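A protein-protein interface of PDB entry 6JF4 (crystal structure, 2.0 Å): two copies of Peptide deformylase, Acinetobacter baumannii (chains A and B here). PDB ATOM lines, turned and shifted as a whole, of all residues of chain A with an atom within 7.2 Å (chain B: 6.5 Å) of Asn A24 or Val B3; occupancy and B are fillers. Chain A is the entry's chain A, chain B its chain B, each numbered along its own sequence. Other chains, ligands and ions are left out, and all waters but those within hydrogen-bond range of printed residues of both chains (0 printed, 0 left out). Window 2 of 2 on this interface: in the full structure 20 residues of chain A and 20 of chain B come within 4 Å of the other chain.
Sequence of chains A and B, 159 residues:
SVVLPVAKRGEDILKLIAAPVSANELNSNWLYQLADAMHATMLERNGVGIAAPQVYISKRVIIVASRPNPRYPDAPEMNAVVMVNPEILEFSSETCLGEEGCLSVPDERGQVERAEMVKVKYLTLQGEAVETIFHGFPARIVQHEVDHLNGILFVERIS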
ATOM      1  N   VAL A  21       0.487  -4.945 -23.451  1.00  0.00           N
ATOM      2  CA  VAL A  21       0.789  -3.744 -22.632  1.00  0.00           C
ATOM      3  C   VAL A  21       1.016  -4.181 -21.176  1.00  0.00           C
ATOM      4  O   VAL A  21       0.270  -5.022 -20.724  1.00  0.00           O
ATOM      5  CB  VAL A  21      -0.351  -2.738 -22.800  1.00  0.00           C
ATOM      6  CG1 VAL A  21      -0.237  -1.589 -21.826  1.00  0.00           C
ATOM      7  CG2 VAL A  21      -0.377  -2.225 -24.237  1.00  0.00           C
ATOM      8  N   SER A  22       2.021  -3.629 -20.489  1.00  0.00           N
ATOM      9  CA  SER A  22       2.354  -3.921 -19.070  1.00  0.00           C
ATOM     10  C   SER A  22       1.417  -3.151 -18.121  1.00  0.00           C
ATOM     11  O   SER A  22       0.848  -2.111 -18.526  1.00  0.00           O
ATOM     12  CB  SER A  22       3.793  -3.577 -18.788  1.00  0.00           C
ATOM     13  OG  SER A  22       3.958  -2.159 -18.741  1.00  0.00           O
ATOM     14  N   ALA A  23       1.304  -3.611 -16.871  1.00  0.00           N
ATOM     15  CA  ALA A  23       0.662  -2.875 -15.756  1.00  0.00           C
ATOM     16  C   ALA A  23       1.296  -1.475 -15.598  1.00  0.00           C
ATOM     17  O   ALA A  23       0.542  -0.500 -15.419  1.00  0.00           O
ATOM     18  CB  ALA A  23       0.738  -3.679 -14.473  1.00  0.00           C
ATOM     19  N   ASN A  24       2.619  -1.351 -15.747  1.00  0.00           N
ATOM     20  CA  ASN A  24       3.338  -0.056 -15.583  1.00  0.00           C
ATOM     21  C   ASN A  24       2.720   0.996 -16.497  1.00  0.00           C
ATOM     22  O   ASN A  24       2.613   2.146 -16.085  1.00  0.00           O
ATOM     23  CB  ASN A  24       4.829  -0.185 -15.896  1.00  0.00           C
ATOM     24  CG  ASN A  24       5.652  -0.698 -14.734  1.00  0.00           C
ATOM     25  OD1 ASN A  24       6.224   0.094 -13.984  1.00  0.00           O
ATOM     26  ND2 ASN A  24       5.750  -2.002 -14.582  1.00  0.00           N
ATOM     27  N   GLU A  25       2.304   0.609 -17.697  1.00  0.00           N
ATOM     28  CA  GLU A  25       1.874   1.567 -18.754  1.00  0.00           C
ATOM     29  C   GLU A  25       0.413   1.986 -18.556  1.00  0.00           C
ATOM     30  O   GLU A  25       0.004   2.989 -19.121  1.00  0.00           O
ATOM     31  CB  GLU A  25       2.002   0.949 -20.145  1.00  0.00           C
ATOM     32  CG  GLU A  25       3.402   0.522 -20.521  1.00  0.00           C
ATOM     33  CD  GLU A  25       3.462  -0.275 -21.820  1.00  0.00           C
ATOM     34  OE1 GLU A  25       3.612  -1.513 -21.749  1.00  0.00           O
ATOM     35  OE2 GLU A  25       3.332   0.366 -22.905  1.00  0.00           O
ATOM     36  N   LEU A  26      -0.387   1.241 -17.807  1.00  0.00           N
ATOM     37  CA  LEU A  26      -1.816   1.632 -17.667  1.00  0.00           C
ATOM     38  C   LEU A  26      -1.911   2.972 -16.921  1.00  0.00           C
ATOM     39  O   LEU A  26      -1.087   3.258 -16.029  1.00  0.00           O
ATOM     40  CB  LEU A  26      -2.590   0.508 -16.992  1.00  0.00           C
ATOM     41  CG  LEU A  26      -2.567  -0.806 -17.766  1.00  0.00           C
ATOM     42  CD1 LEU A  26      -2.931  -1.973 -16.854  1.00  0.00           C
ATOM     43  CD2 LEU A  26      -3.444  -0.742 -19.012  1.00  0.00           C
ATOM     44  N   ASN A  27      -2.816   3.814 -17.377  1.00  0.00           N
ATOM     45  CA  ASN A  27      -3.134   5.128 -16.776  1.00  0.00           C
ATOM     46  C   ASN A  27      -1.904   6.049 -16.829  1.00  0.00           C
ATOM     47  O   ASN A  27      -1.755   6.877 -15.912  1.00  0.00           O
ATOM     48  CB  ASN A  27      -3.701   4.954 -15.369  1.00  0.00           C
ATOM     49  CG  ASN A  27      -4.431   6.197 -14.918  1.00  0.00           C
ATOM     50  OD1 ASN A  27      -4.083   6.751 -13.884  1.00  0.00           O
ATOM     51  ND2 ASN A  27      -5.342   6.705 -15.739  1.00  0.00           N
ATOM     52  N   SER A  28      -1.069   5.921 -17.868  1.00  0.00           N
ATOM     53  CA  SER A  28       0.162   6.731 -18.066  1.00  0.00           C
ATOM     54  C   SER A  28      -0.053   7.771 -19.178  1.00  0.00           C
ATOM     55  O   SER A  28      -0.832   7.526 -20.126  1.00  0.00           O
ATOM     56  CB  SER A  28       1.347   5.861 -18.355  1.00  0.00           C
ATOM     57  OG  SER A  28       1.256   5.243 -19.639  1.00  0.00           O
ATOM     58  N   TRP A  30       2.143   8.279 -21.340  1.00  0.00           N
ATOM     59  CA  TRP A  30       2.679   7.493 -22.479  1.00  0.00           C
ATOM     60  C   TRP A  30       1.511   6.820 -23.218  1.00  0.00           C
ATOM     61  O   TRP A  30       1.359   6.995 -24.435  1.00  0.00           O
ATOM     62  CB  TRP A  30       3.747   6.502 -21.986  1.00  0.00           C
ATOM     63  CG  TRP A  30       3.833   5.272 -22.822  1.00  0.00           C
ATOM     64  CD1 TRP A  30       3.478   4.014 -22.439  1.00  0.00           C
ATOM     65  CD2 TRP A  30       4.223   5.169 -24.205  1.00  0.00           C
ATOM     66  NE1 TRP A  30       3.657   3.137 -23.469  1.00  0.00           N
ATOM     67  CE2 TRP A  30       4.103   3.809 -24.565  1.00  0.00           C
ATOM     68  CE3 TRP A  30       4.667   6.080 -25.167  1.00  0.00           C
ATOM     69  CZ2 TRP A  30       4.400   3.339 -25.841  1.00  0.00           C
ATOM     70  CZ3 TRP A  30       4.950   5.621 -26.436  1.00  0.00           C
ATOM     71  CH2 TRP A  30       4.814   4.270 -26.767  1.00  0.00           C
ATOM     72  N   SER B   1       6.685   9.232 -14.908  1.00  0.00           N
ATOM     73  CA  SER B   1       7.666   8.382 -15.643  1.00  0.00           C
ATOM     74  C   SER B   1       7.202   6.922 -15.624  1.00  0.00           C
ATOM     75  O   SER B   1       6.888   6.425 -14.542  1.00  0.00           O
ATOM     76  CB  SER B   1       9.023   8.521 -15.046  1.00  0.00           C
ATOM     77  OG  SER B   1       9.577   9.769 -15.409  1.00  0.00           O
ATOM     78  N   VAL B   2       7.155   6.263 -16.783  1.00  0.00           N
ATOM     79  CA  VAL B   2       6.743   4.840 -16.910  1.00  0.00           C
ATOM     80  C   VAL B   2       7.944   3.973 -17.275  1.00  0.00           C
ATOM     81  O   VAL B   2       8.680   4.304 -18.233  1.00  0.00           O
ATOM     82  CB  VAL B   2       5.634   4.720 -17.960  1.00  0.00           C
ATOM     83  CG1 VAL B   2       5.317   3.275 -18.282  1.00  0.00           C
ATOM     84  CG2 VAL B   2       4.392   5.455 -17.509  1.00  0.00           C
ATOM     85  N   VAL B   3       8.097   2.855 -16.583  1.00  0.00           N
ATOM     86  CA  VAL B   3       9.075   1.786 -16.935  1.00  0.00           C
ATOM     87  C   VAL B   3       8.393   0.810 -17.893  1.00  0.00           C
ATOM     88  O   VAL B   3       7.377   0.220 -17.518  1.00  0.00           O
ATOM     89  CB  VAL B   3       9.590   1.076 -15.672  1.00  0.00           C
ATOM     90  CG1 VAL B   3      10.433  -0.147 -16.008  1.00  0.00           C
ATOM     91  CG2 VAL B   3      10.366   2.046 -14.790  1.00  0.00           C
ATOM     92  N   LEU B   4       8.913   0.675 -19.106  1.00  0.00           N
ATOM     93  CA  LEU B   4       8.271  -0.150 -20.169  1.00  0.00           C
ATOM     94  C   LEU B   4       8.859  -1.549 -20.137  1.00  0.00           C
ATOM     95  O   LEU B   4      10.005  -1.719 -19.727  1.00  0.00           O
ATOM     96  CB  LEU B   4       8.557   0.494 -21.525  1.00  0.00           C
ATOM     97  CG  LEU B   4       8.018   1.899 -21.771  1.00  0.00           C
ATOM     98  CD1 LEU B   4       8.524   2.416 -23.107  1.00  0.00           C
ATOM     99  CD2 LEU B   4       6.515   1.902 -21.772  1.00  0.00           C
ATOM    100  N   PRO B   5       8.110  -2.581 -20.573  1.00  0.00           N
ATOM    101  CA  PRO B   5       8.680  -3.908 -20.776  1.00  0.00           C
ATOM    102  C   PRO B   5       9.745  -3.915 -21.884  1.00  0.00           C
ATOM    103  O   PRO B   5       9.657  -3.139 -22.831  1.00  0.00           O
ATOM    104  CB  PRO B   5       7.484  -4.796 -21.146  1.00  0.00           C
ATOM    105  CG  PRO B   5       6.441  -3.830 -21.650  1.00  0.00           C
ATOM    106  CD  PRO B   5       6.689  -2.525 -20.925  1.00  0.00           C
ATOM    107  N   ALA B  37       9.730   7.770 -21.306  1.00  0.00           N
ATOM    108  CA  ALA B  37       9.441   6.377 -20.896  1.00  0.00           C
ATOM    109  C   ALA B  37      10.666   5.485 -21.214  1.00  0.00           C
ATOM    110  O   ALA B  37      11.089   4.671 -20.336  1.00  0.00           O
ATOM    111  CB  ALA B  37       8.161   5.970 -21.563  1.00  0.00           C
ATOM    112  N   ALA B  40      13.245   6.444 -18.426  1.00  0.00           N
ATOM    113  CA  ALA B  40      12.859   5.777 -17.164  1.00  0.00           C
ATOM    114  C   ALA B  40      13.239   4.301 -17.249  1.00  0.00           C
ATOM    115  O   ALA B  40      13.812   3.772 -16.284  1.00  0.00           O
ATOM    116  CB  ALA B  40      11.387   5.961 -16.853  1.00  0.00           C
ATOM    117  N   THR B  41      12.976   3.649 -18.381  1.00  0.00           N
ATOM    118  CA  THR B  41      13.301   2.211 -18.552  1.00  0.00           C
ATOM    119  C   THR B  41      14.806   1.994 -18.401  1.00  0.00           C
ATOM    120  O   THR B  41      15.216   1.044 -17.682  1.00  0.00           O
ATOM    121  CB  THR B  41      12.760   1.645 -19.868  1.00  0.00           C
ATOM    122  OG1 THR B  41      11.362   1.937 -19.879  1.00  0.00           O
ATOM    123  CG2 THR B  41      12.999   0.152 -19.954  1.00  0.00           C
ATOM    124  N   GLU B  44      15.828   2.479 -14.654  1.00  0.00           N
ATOM    125  CA  GLU B  44      15.326   1.304 -13.889  1.00  0.00           C
ATOM    126  C   GLU B  44      16.335   0.160 -13.889  1.00  0.00           C
ATOM    127  O   GLU B  44      16.398  -0.572 -12.907  1.00  0.00           O
ATOM    128  CB  GLU B  44      14.055   0.778 -14.549  1.00  0.00           C
ATOM    129  CG  GLU B  44      13.689  -0.657 -14.174  1.00  0.00           C
ATOM    130  CD  GLU B  44      13.041  -0.688 -12.811  1.00  0.00           C
ATOM    131  OE1 GLU B  44      12.865   0.419 -12.261  1.00  0.00           O
ATOM    132  OE2 GLU B  44      12.700  -1.805 -12.320  1.00  0.00           O
ATOM    133  N   ARG B  45      17.019  -0.060 -15.011  1.00  0.00           N
ATOM    134  CA  ARG B  45      17.913  -1.217 -15.228  1.00  0.00           C
ATOM    135  C   ARG B  45      19.368  -0.787 -15.070  1.00  0.00           C
ATOM    136  O   ARG B  45      20.238  -1.573 -15.417  1.00  0.00           O
ATOM    137  CB  ARG B  45      17.659  -1.757 -16.636  1.00  0.00           C
ATOM    138  CG  ARG B  45      16.215  -2.159 -16.894  1.00  0.00           C
ATOM    139  CD  ARG B  45      15.918  -3.426 -16.102  1.00  0.00           C
ATOM    140  NE  ARG B  45      14.804  -4.202 -16.641  1.00  0.00           N
ATOM    141  CZ  ARG B  45      14.818  -4.914 -17.778  1.00  0.00           C
ATOM    142  NH1 ARG B  45      13.736  -5.595 -18.140  1.00  0.00           N
ATOM    143  NH2 ARG B  45      15.905  -4.964 -18.537  1.00  0.00           N
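Printed residues of chain B within 4 Å of Ser A22: Pro B5. Asn A24 touches just these residues of chain B: Val B2 and Val B3. Printed residues of chain B within 4 Å of Glu A25: Val B2 (3.9 Å), Leu B4 (3.6 Å) and Pro B5 (3.3 Å). Val B3 touches just one residue of chain A: Asn A24. Ala B37 touches none of the printed residues of chain A.
No position is printed for both chains.
Among the printed residues, merely in contact across the chains: Ser A22 with Pro B5, Asn A24 with Val B2, Asn A24 with Val B3, Glu A25 with Val B2, Glu A25 with Leu B4, Glu A25 with Pro B5, Ser A28 with Val B2 and Trp A30 with Leu B4.
The backbone NH of Leu B4 lies within hydrogen-bond range of the side-chain hydroxyl of Thr B41, at 2.9 Å. The side-chain hydroxyl (OG) of Ser A22 lies close to the backbone NH (N) of Asn A24 (3.4 Å). The side-chain carboxylate of Glu A25 lies within hydrogen-bond range of the backbone NH of Ser A22 (2.9 Å). OG of Ser A28 is in hydrogen-bond range of O of Glu A25. The indole nitrogen (NE1) of Trp A30 is in hydrogen-bond range of the side-chain carboxylate (OE2) of Glu A25.
Of the 9 printed residues of chain A, 5 touch a printed residue of chain B. Of the 10 printed residues of chain B, 4 touch a printed residue of chain A. Printed residues of chain B that touch a printed residue of chain A: Val B2, Val B3, Leu B4 and Pro B5. Among the printed residues, 8 pairs touch across the chains. Among the printed residues, no Asp or Glu carboxylate lies within 4 Å of a Lys or Arg side-chain nitrogen of the other chain.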
